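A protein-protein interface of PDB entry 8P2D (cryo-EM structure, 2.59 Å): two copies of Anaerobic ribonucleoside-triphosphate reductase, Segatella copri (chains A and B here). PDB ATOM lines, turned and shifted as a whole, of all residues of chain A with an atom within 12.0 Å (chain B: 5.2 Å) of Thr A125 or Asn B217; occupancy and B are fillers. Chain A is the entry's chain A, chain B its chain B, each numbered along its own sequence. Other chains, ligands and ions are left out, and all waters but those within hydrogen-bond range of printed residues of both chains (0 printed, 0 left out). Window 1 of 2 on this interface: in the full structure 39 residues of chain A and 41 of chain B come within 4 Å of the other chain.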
ATOM      1  N   ASP A 124     -26.630 -32.149  17.340  1.00  0.00           N
ATOM      2  CA  ASP A 124     -25.238 -32.376  16.971  1.00  0.00           C
ATOM      3  C   ASP A 124     -24.835 -31.520  15.774  1.00  0.00           C
ATOM      4  O   ASP A 124     -23.879 -30.747  15.847  1.00  0.00           O
ATOM      5  CB  ASP A 124     -25.001 -33.857  16.664  1.00  0.00           C
ATOM      6  CG  ASP A 124     -25.114 -34.734  17.896  1.00  0.00           C
ATOM      7  OD1 ASP A 124     -24.811 -34.248  19.006  1.00  0.00           O
ATOM      8  OD2 ASP A 124     -25.503 -35.912  17.754  1.00  0.00           O
ATOM      9  N   THR A 125     -25.566 -31.672  14.674  1.00  0.00           N
ATOM     10  CA  THR A 125     -25.278 -30.894  13.478  1.00  0.00           C
ATOM     11  C   THR A 125     -25.564 -29.416  13.731  1.00  0.00           C
ATOM     12  O   THR A 125     -26.588 -29.077  14.334  1.00  0.00           O
ATOM     13  CB  THR A 125     -26.114 -31.400  12.299  1.00  0.00           C
ATOM     14  OG1 THR A 125     -25.827 -32.785  12.072  1.00  0.00           O
ATOM     15  CG2 THR A 125     -25.800 -30.615  11.033  1.00  0.00           C
ATOM     16  N   PRO A 126     -24.673 -28.514  13.305  1.00  0.00           N
ATOM     17  CA  PRO A 126     -24.953 -27.079  13.483  1.00  0.00           C
ATOM     18  C   PRO A 126     -26.258 -26.637  12.846  1.00  0.00           C
ATOM     19  O   PRO A 126     -26.976 -25.814  13.427  1.00  0.00           O
ATOM     20  CB  PRO A 126     -23.740 -26.407  12.827  1.00  0.00           C
ATOM     21  CG  PRO A 126     -22.652 -27.416  12.931  1.00  0.00           C
ATOM     22  CD  PRO A 126     -23.317 -28.754  12.778  1.00  0.00           C
ATOM     23  N   ALA A 127     -26.592 -27.170  11.668  1.00  0.00           N
ATOM     24  CA  ALA A 127     -27.866 -26.843  11.042  1.00  0.00           C
ATOM     25  C   ALA A 127     -29.049 -27.339  11.860  1.00  0.00           C
ATOM     26  O   ALA A 127     -30.079 -26.660  11.913  1.00  0.00           O
ATOM     27  CB  ALA A 127     -27.929 -27.424   9.630  1.00  0.00           C
ATOM     28  N   GLY A 128     -28.924 -28.499  12.498  1.00  0.00           N
ATOM     29  CA  GLY A 128     -29.972 -28.991  13.363  1.00  0.00           C
ATOM     30  C   GLY A 128     -30.101 -28.164  14.623  1.00  0.00           C
ATOM     31  O   GLY A 128     -31.213 -27.876  15.073  1.00  0.00           O
ATOM     32  N   MET A 129     -28.964 -27.771  15.199  1.00  0.00           N
ATOM     33  CA  MET A 129     -28.959 -26.943  16.399  1.00  0.00           C
ATOM     34  C   MET A 129     -29.557 -25.565  16.154  1.00  0.00           C
ATOM     35  O   MET A 129     -30.286 -25.049  17.007  1.00  0.00           O
ATOM     36  CB  MET A 129     -27.534 -26.805  16.940  1.00  0.00           C
ATOM     37  CG  MET A 129     -26.942 -28.105  17.459  1.00  0.00           C
ATOM     38  SD  MET A 129     -25.291 -27.889  18.146  1.00  0.00           S
ATOM     39  CE  MET A 129     -25.613 -26.660  19.408  1.00  0.00           C
ATOM     40  N   MET A 130     -29.264 -24.957  15.001  1.00  0.00           N
ATOM     41  CA  MET A 130     -29.857 -23.662  14.682  1.00  0.00           C
ATOM     42  C   MET A 130     -31.372 -23.765  14.546  1.00  0.00           C
ATOM     43  O   MET A 130     -32.106 -22.903  15.041  1.00  0.00           O
ATOM     44  CB  MET A 130     -29.238 -23.101  13.402  1.00  0.00           C
ATOM     45  CG  MET A 130     -27.761 -22.773  13.522  1.00  0.00           C
ATOM     46  SD  MET A 130     -27.412 -21.505  14.752  1.00  0.00           S
ATOM     47  CE  MET A 130     -25.625 -21.547  14.771  1.00  0.00           C
ATOM     48  N   MET A 131     -31.860 -24.815  13.879  1.00  0.00           N
ATOM     49  CA  MET A 131     -33.303 -24.996  13.747  1.00  0.00           C
ATOM     50  C   MET A 131     -33.952 -25.276  15.095  1.00  0.00           C
ATOM     51  O   MET A 131     -35.055 -24.789  15.373  1.00  0.00           O
ATOM     52  CB  MET A 131     -33.605 -26.120  12.759  1.00  0.00           C
ATOM     53  CG  MET A 131     -33.227 -25.798  11.324  1.00  0.00           C
ATOM     54  SD  MET A 131     -34.093 -24.350  10.686  1.00  0.00           S
ATOM     55  CE  MET A 131     -33.427 -24.259   9.027  1.00  0.00           C
ATOM     56  N   LYS A 132     -33.287 -26.060  15.946  1.00  0.00           N
ATOM     57  CA  LYS A 132     -33.820 -26.321  17.279  1.00  0.00           C
ATOM     58  C   LYS A 132     -33.898 -25.041  18.102  1.00  0.00           C
ATOM     59  O   LYS A 132     -34.890 -24.800  18.800  1.00  0.00           O
ATOM     60  CB  LYS A 132     -32.962 -27.372  17.984  1.00  0.00           C
ATOM     61  CG  LYS A 132     -33.556 -27.900  19.277  1.00  0.00           C
ATOM     62  CD  LYS A 132     -32.708 -29.020  19.854  1.00  0.00           C
ATOM     63  CE  LYS A 132     -33.308 -29.566  21.139  1.00  0.00           C
ATOM     64  NZ  LYS A 132     -33.423 -28.514  22.187  1.00  0.00           N
ATOM     65  N   PHE A 133     -32.863 -24.200  18.023  1.00  0.00           N
ATOM     66  CA  PHE A 133     -32.889 -22.921  18.727  1.00  0.00           C
ATOM     67  C   PHE A 133     -33.984 -22.013  18.184  1.00  0.00           C
ATOM     68  O   PHE A 133     -34.669 -21.327  18.951  1.00  0.00           O
ATOM     69  CB  PHE A 133     -31.527 -22.237  18.624  1.00  0.00           C
ATOM     70  CG  PHE A 133     -30.509 -22.763  19.594  1.00  0.00           C
ATOM     71  CD1 PHE A 133     -30.905 -23.462  20.722  1.00  0.00           C
ATOM     72  CD2 PHE A 133     -29.158 -22.555  19.381  1.00  0.00           C
ATOM     73  CE1 PHE A 133     -29.971 -23.945  21.617  1.00  0.00           C
ATOM     74  CE2 PHE A 133     -28.219 -23.036  20.272  1.00  0.00           C
ATOM     75  CZ  PHE A 133     -28.627 -23.732  21.392  1.00  0.00           C
ATOM     76  N   ALA A 134     -34.160 -21.990  16.861  1.00  0.00           N
ATOM     77  CA  ALA A 134     -35.223 -21.185  16.272  1.00  0.00           C
ATOM     78  C   ALA A 134     -36.591 -21.648  16.755  1.00  0.00           C
ATOM     79  O   ALA A 134     -37.448 -20.825  17.098  1.00  0.00           O
ATOM     80  CB  ALA A 134     -35.142 -21.242  14.748  1.00  0.00           C
ATOM     81  N   TYR A 167     -43.777 -21.980  12.822  1.00  0.00           N
ATOM     82  CA  TYR A 167     -43.837 -21.070  11.677  1.00  0.00           C
ATOM     83  C   TYR A 167     -45.150 -20.292  11.638  1.00  0.00           C
ATOM     84  O   TYR A 167     -45.792 -20.182  10.596  1.00  0.00           O
ATOM     85  CB  TYR A 167     -43.642 -21.852  10.385  1.00  0.00           C
ATOM     86  CG  TYR A 167     -42.245 -22.384  10.154  1.00  0.00           C
ATOM     87  CD1 TYR A 167     -41.715 -23.378  10.961  1.00  0.00           C
ATOM     88  CD2 TYR A 167     -41.466 -21.908   9.108  1.00  0.00           C
ATOM     89  CE1 TYR A 167     -40.445 -23.869  10.747  1.00  0.00           C
ATOM     90  CE2 TYR A 167     -40.194 -22.395   8.887  1.00  0.00           C
ATOM     91  CZ  TYR A 167     -39.689 -23.375   9.708  1.00  0.00           C
ATOM     92  OH  TYR A 167     -38.422 -23.864   9.492  1.00  0.00           O
ATOM     93  N   GLU A 213     -37.441 -27.376  -3.024  1.00  0.00           N
ATOM     94  CA  GLU A 213     -36.557 -26.910  -1.963  1.00  0.00           C
ATOM     95  C   GLU A 213     -36.778 -25.441  -1.624  1.00  0.00           C
ATOM     96  O   GLU A 213     -36.720 -25.067  -0.447  1.00  0.00           O
ATOM     97  CB  GLU A 213     -35.099 -27.139  -2.361  1.00  0.00           C
ATOM     98  CG  GLU A 213     -34.724 -28.598  -2.526  1.00  0.00           C
ATOM     99  CD  GLU A 213     -33.301 -28.779  -3.010  1.00  0.00           C
ATOM    100  OE1 GLU A 213     -32.683 -27.777  -3.425  1.00  0.00           O
ATOM    101  OE2 GLU A 213     -32.799 -29.922  -2.972  1.00  0.00           O
ATOM    102  N   GLN A 216     -39.982 -25.093   0.213  1.00  0.00           N
ATOM    103  CA  GLN A 216     -39.820 -25.622   1.561  1.00  0.00           C
ATOM    104  C   GLN A 216     -39.249 -24.571   2.501  1.00  0.00           C
ATOM    105  O   GLN A 216     -39.507 -24.614   3.709  1.00  0.00           O
ATOM    106  CB  GLN A 216     -38.927 -26.861   1.535  1.00  0.00           C
ATOM    107  CG  GLN A 216     -38.841 -27.591   2.865  1.00  0.00           C
ATOM    108  CD  GLN A 216     -40.199 -28.028   3.376  1.00  0.00           C
ATOM    109  OE1 GLN A 216     -40.795 -27.373   4.227  1.00  0.00           O
ATOM    110  NE2 GLN A 216     -40.693 -29.144   2.855  1.00  0.00           N
ATOM    111  N   ASN A 217     -38.482 -23.619   1.970  1.00  0.00           N
ATOM    112  CA  ASN A 217     -37.983 -22.513   2.773  1.00  0.00           C
ATOM    113  C   ASN A 217     -39.039 -21.446   3.019  1.00  0.00           C
ATOM    114  O   ASN A 217     -38.808 -20.544   3.830  1.00  0.00           O
ATOM    115  CB  ASN A 217     -36.764 -21.883   2.097  1.00  0.00           C
ATOM    116  CG  ASN A 217     -35.634 -22.872   1.903  1.00  0.00           C
ATOM    117  OD1 ASN A 217     -35.440 -23.776   2.713  1.00  0.00           O
ATOM    118  ND2 ASN A 217     -34.880 -22.704   0.822  1.00  0.00           N
ATOM    119  N   ASN A 302     -31.471 -36.883  -4.189  1.00  0.00           N
ATOM    120  CA  ASN A 302     -31.520 -35.481  -3.800  1.00  0.00           C
ATOM    121  C   ASN A 302     -32.612 -35.241  -2.768  1.00  0.00           C
ATOM    122  O   ASN A 302     -32.450 -34.419  -1.859  1.00  0.00           O
ATOM    123  CB  ASN A 302     -31.737 -34.606  -5.035  1.00  0.00           C
ATOM    124  CG  ASN A 302     -31.450 -33.142  -4.772  1.00  0.00           C
ATOM    125  OD1 ASN A 302     -32.327 -32.393  -4.344  1.00  0.00           O
ATOM    126  ND2 ASN A 302     -30.217 -32.726  -5.031  1.00  0.00           N
ATOM    127  N   THR A 305     -31.290 -36.941   0.650  1.00  0.00           N
ATOM    128  CA  THR A 305     -30.078 -36.404   1.251  1.00  0.00           C
ATOM    129  C   THR A 305     -30.417 -35.141   2.028  1.00  0.00           C
ATOM    130  O   THR A 305     -31.084 -34.244   1.503  1.00  0.00           O
ATOM    131  CB  THR A 305     -29.019 -36.102   0.187  1.00  0.00           C
ATOM    132  OG1 THR A 305     -28.670 -37.312  -0.496  1.00  0.00           O
ATOM    133  CG2 THR A 305     -27.772 -35.511   0.826  1.00  0.00           C
ATOM    134  N   ILE A 306     -29.958 -35.077   3.274  1.00  0.00           N
ATOM    135  CA  ILE A 306     -30.204 -33.922   4.125  1.00  0.00           C
ATOM    136  C   ILE A 306     -29.347 -32.747   3.671  1.00  0.00           C
ATOM    137  O   ILE A 306     -28.118 -32.810   3.713  1.00  0.00           O
ATOM    138  CB  ILE A 306     -29.937 -34.247   5.611  1.00  0.00           C
ATOM    139  CG1 ILE A 306     -30.946 -35.276   6.134  1.00  0.00           C
ATOM    140  CG2 ILE A 306     -29.983 -32.981   6.450  1.00  0.00           C
ATOM    141  CD1 ILE A 306     -30.505 -36.718   5.977  1.00  0.00           C
ATOM    142  N   VAL A 315     -36.289 -32.732   3.299  1.00  0.00           N
ATOM    143  CA  VAL A 315     -37.413 -32.189   2.550  1.00  0.00           C
ATOM    144  C   VAL A 315     -38.523 -33.228   2.447  1.00  0.00           C
ATOM    145  O   VAL A 315     -38.298 -34.346   1.984  1.00  0.00           O
ATOM    146  CB  VAL A 315     -36.977 -31.713   1.155  1.00  0.00           C
ATOM    147  CG1 VAL A 315     -38.162 -31.155   0.389  1.00  0.00           C
ATOM    148  CG2 VAL A 315     -35.879 -30.668   1.273  1.00  0.00           C
ATOM    149  N   GLU B 213     -22.827 -27.931  -0.265  1.00  0.00           N
ATOM    150  CA  GLU B 213     -24.057 -27.569   0.433  1.00  0.00           C
ATOM    151  C   GLU B 213     -24.146 -28.249   1.796  1.00  0.00           C
ATOM    152  O   GLU B 213     -24.470 -27.605   2.801  1.00  0.00           O
ATOM    153  CB  GLU B 213     -25.269 -27.927  -0.427  1.00  0.00           C
ATOM    154  CG  GLU B 213     -25.421 -27.074  -1.674  1.00  0.00           C
ATOM    155  CD  GLU B 213     -26.613 -27.484  -2.516  1.00  0.00           C
ATOM    156  OE1 GLU B 213     -27.220 -28.535  -2.217  1.00  0.00           O
ATOM    157  OE2 GLU B 213     -26.945 -26.756  -3.474  1.00  0.00           O
ATOM    158  N   THR B 214     -23.872 -29.555   1.847  1.00  0.00           N
ATOM    159  CA  THR B 214     -23.971 -30.298   3.099  1.00  0.00           C
ATOM    160  C   THR B 214     -22.945 -29.817   4.114  1.00  0.00           C
ATOM    161  O   THR B 214     -23.262 -29.658   5.298  1.00  0.00           O
ATOM    162  CB  THR B 214     -23.797 -31.794   2.835  1.00  0.00           C
ATOM    163  OG1 THR B 214     -24.794 -32.236   1.906  1.00  0.00           O
ATOM    164  CG2 THR B 214     -23.929 -32.585   4.125  1.00  0.00           C
ATOM    165  N   CYS B 215     -21.708 -29.580   3.672  1.00  0.00           N
ATOM    166  CA  CYS B 215     -20.686 -29.077   4.579  1.00  0.00           C
ATOM    167  C   CYS B 215     -21.015 -27.674   5.061  1.00  0.00           C
ATOM    168  O   CYS B 215     -20.658 -27.305   6.185  1.00  0.00           O
ATOM    169  CB  CYS B 215     -19.322 -29.108   3.892  1.00  0.00           C
ATOM    170  SG  CYS B 215     -17.920 -29.180   5.020  1.00  0.00           S
ATOM    171  N   GLN B 216     -21.691 -26.878   4.230  1.00  0.00           N
ATOM    172  CA  GLN B 216     -22.147 -25.564   4.661  1.00  0.00           C
ATOM    173  C   GLN B 216     -23.131 -25.657   5.816  1.00  0.00           C
ATOM    174  O   GLN B 216     -23.194 -24.739   6.640  1.00  0.00           O
ATOM    175  CB  GLN B 216     -22.784 -24.815   3.489  1.00  0.00           C
ATOM    176  CG  GLN B 216     -23.092 -23.352   3.770  1.00  0.00           C
ATOM    177  CD  GLN B 216     -21.841 -22.511   3.935  1.00  0.00           C
ATOM    178  OE1 GLN B 216     -21.306 -21.980   2.965  1.00  0.00           O
ATOM    179  NE2 GLN B 216     -21.369 -22.386   5.169  1.00  0.00           N
ATOM    180  N   ASN B 217     -23.897 -26.742   5.898  1.00  0.00           N
ATOM    181  CA  ASN B 217     -24.782 -26.967   7.030  1.00  0.00           C
ATOM    182  C   ASN B 217     -24.034 -27.396   8.286  1.00  0.00           C
ATOM    183  O   ASN B 217     -24.630 -27.408   9.368  1.00  0.00           O
ATOM    184  CB  ASN B 217     -25.837 -28.016   6.673  1.00  0.00           C
ATOM    185  CG  ASN B 217     -26.789 -27.539   5.597  1.00  0.00           C
ATOM    186  OD1 ASN B 217     -27.817 -26.929   5.889  1.00  0.00           O
ATOM    187  ND2 ASN B 217     -26.452 -27.815   4.343  1.00  0.00           N
ATOM    188  N   GLU B 218     -22.753 -27.739   8.172  1.00  0.00           N
ATOM    189  CA  GLU B 218     -21.948 -28.125   9.318  1.00  0.00           C
ATOM    190  C   GLU B 218     -20.800 -27.167   9.594  1.00  0.00           C
ATOM    191  O   GLU B 218     -19.965 -27.462  10.454  1.00  0.00           O
ATOM    192  CB  GLU B 218     -21.394 -29.543   9.124  1.00  0.00           C
ATOM    193  CG  GLU B 218     -22.468 -30.613   9.003  1.00  0.00           C
ATOM    194  CD  GLU B 218     -22.359 -31.409   7.719  1.00  0.00           C
ATOM    195  OE1 GLU B 218     -21.372 -31.213   6.979  1.00  0.00           O
ATOM    196  OE2 GLU B 218     -23.258 -32.231   7.449  1.00  0.00           O
ATOM    197  N   MET B 219     -20.730 -26.039   8.892  1.00  0.00           N
ATOM    198  CA  MET B 219     -19.692 -25.041   9.097  1.00  0.00           C
ATOM    199  C   MET B 219     -20.302 -23.658   8.937  1.00  0.00           C
ATOM    200  O   MET B 219     -21.357 -23.494   8.319  1.00  0.00           O
ATOM    201  CB  MET B 219     -18.528 -25.232   8.119  1.00  0.00           C
ATOM    202  CG  MET B 219     -17.630 -26.406   8.454  1.00  0.00           C
ATOM    203  SD  MET B 219     -16.543 -26.834   7.092  1.00  0.00           S
ATOM    204  CE  MET B 219     -16.213 -25.219   6.408  1.00  0.00           C
ATOM    205  N   LYS B 495     -19.379 -37.614  14.746  1.00  0.00           N
ATOM    206  CA  LYS B 495     -20.751 -37.677  14.266  1.00  0.00           C
ATOM    207  C   LYS B 495     -21.525 -36.384  14.487  1.00  0.00           C
ATOM    208  O   LYS B 495     -22.672 -36.286  14.036  1.00  0.00           O
ATOM    209  CB  LYS B 495     -21.490 -38.835  14.943  1.00  0.00           C
ATOM    210  CG  LYS B 495     -21.509 -38.751  16.459  1.00  0.00           C
ATOM    211  CD  LYS B 495     -22.248 -39.930  17.070  1.00  0.00           C
ATOM    212  CE  LYS B 495     -22.284 -39.834  18.588  1.00  0.00           C
ATOM    213  NZ  LYS B 495     -22.989 -40.992  19.202  1.00  0.00           N
ATOM    214  N   GLN B 496     -20.941 -35.396  15.173  1.00  0.00           N
ATOM    215  CA  GLN B 496     -21.623 -34.115  15.328  1.00  0.00           C
ATOM    216  C   GLN B 496     -21.826 -33.435  13.982  1.00  0.00           C
ATOM    217  O   GLN B 496     -22.929 -32.975  13.670  1.00  0.00           O
ATOM    218  CB  GLN B 496     -20.844 -33.200  16.270  1.00  0.00           C
ATOM    219  CG  GLN B 496     -21.122 -33.435  17.737  1.00  0.00           C
ATOM    220  CD  GLN B 496     -20.864 -32.200  18.573  1.00  0.00           C
ATOM    221  OE1 GLN B 496     -20.832 -31.085  18.057  1.00  0.00           O
ATOM    222  NE2 GLN B 496     -20.680 -32.394  19.873  1.00  0.00           N
ATOM    223  N   PHE B 497     -20.775 -33.371  13.165  1.00  0.00           N
ATOM    224  CA  PHE B 497     -20.854 -32.825  11.813  1.00  0.00           C
ATOM    225  C   PHE B 497     -20.515 -33.944  10.841  1.00  0.00           C
ATOM    226  O   PHE B 497     -19.332 -34.229  10.596  1.00  0.00           O
ATOM    227  CB  PHE B 497     -19.921 -31.629  11.636  1.00  0.00           C
ATOM    228  CG  PHE B 497     -18.818 -31.559  12.649  1.00  0.00           C
ATOM    229  CD1 PHE B 497     -17.661 -32.297  12.488  1.00  0.00           C
ATOM    230  CD2 PHE B 497     -18.935 -30.747  13.759  1.00  0.00           C
ATOM    231  CE1 PHE B 497     -16.647 -32.228  13.418  1.00  0.00           C
ATOM    232  CE2 PHE B 497     -17.927 -30.681  14.691  1.00  0.00           C
ATOM    233  CZ  PHE B 497     -16.780 -31.420  14.519  1.00  0.00           C
ATOM    234  N   PRO B 498     -21.516 -34.616  10.279  1.00  0.00           N
ATOM    235  CA  PRO B 498     -21.234 -35.677   9.310  1.00  0.00           C
ATOM    236  C   PRO B 498     -20.541 -35.120   8.077  1.00  0.00           C
ATOM    237  O   PRO B 498     -20.729 -33.960   7.702  1.00  0.00           O
ATOM    238  CB  PRO B 498     -22.622 -36.232   8.972  1.00  0.00           C
ATOM    239  CG  PRO B 498     -23.490 -35.827  10.123  1.00  0.00           C
ATOM    240  CD  PRO B 498     -22.953 -34.503  10.573  1.00  0.00           C
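ND2 of Asn B217 lies within hydrogen-bond range of O of Glu B213 (2.5 Å).
The backbone NH of Thr A125 sits at hydrogen-bond distance from the backbone carbonyl oxygen of Gln B496 (3.1 Å).
N of Ala A127 is in hydrogen-bond range of O of Asn B217 (3.0 Å).
The backbone carbonyl oxygen (O) of Gln B496 sits close to the backbone carbonyl oxygen (O) of Asp A124 (3.3 Å).
Of the 19 printed residues of chain A, 5 touch a printed residue of chain B.
Of the 11 printed residues of chain B, 5 touch a printed residue of chain A.
Along chain B the printed residues that touch a printed residue of chain A span positions 214 to 498.
Among the printed residues, no Asp or Glu carboxylate lies within 4 Å of a Lys or Arg side-chain nitrogen of the other chain.
Thr A125 touches just these residues of chain B: Asn B217 (3.8 Å), Glu B218 (3.9 Å), Gln B496 (3.1 Å) and Pro B498 (3.7 Å).
Printed residues of chain B within 4 Å of Ala A127: Asn B217.
Met A129 touches none of the printed residues of chain B.
Met A130 touches none of the printed residues of chain B.
Printed residues of chain B within 4 Å of Ile A306: Thr B214 (3.8 Å).
No residue of chain A comes within 4 Å of Cys B215.
No residue of chain A comes within 4 Å of Gln B216.
Printed residues of chain A within 4 Å of Asn B217: Thr A125 (3.8 Å), Pro A126 (3.7 Å) and Ala A127 (3.0 Å).
Glu B218 touches just these residues of chain A: Thr A125 and Pro A126.
No residue of chain A comes within 4 Å of Met B219.
Gln B496 touches just these residues of chain A: Asp A124 (3.2 Å) and Thr A125 (3.1 Å).
Of chain A, only Thr A125 comes within 4 Å of Pro B498.
The nearest printed residue of chain B that does not touch Ala A127 is Glu B218 (5.2 Å).
Positions printed for both chains: 213, 216 and 217.
Of the 9 pairs that touch across the chains among the printed residues, none has its exchanged pair printed and touching as well.
Among the printed residues, merely in contact across the chains: Pro A126 with Glu B218, Thr A125 with Pro B498, Pro A126 with Asn B217, Thr A125 with Asn B217, Ile A306 with Thr B214 and Thr A125 with Glu B218.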
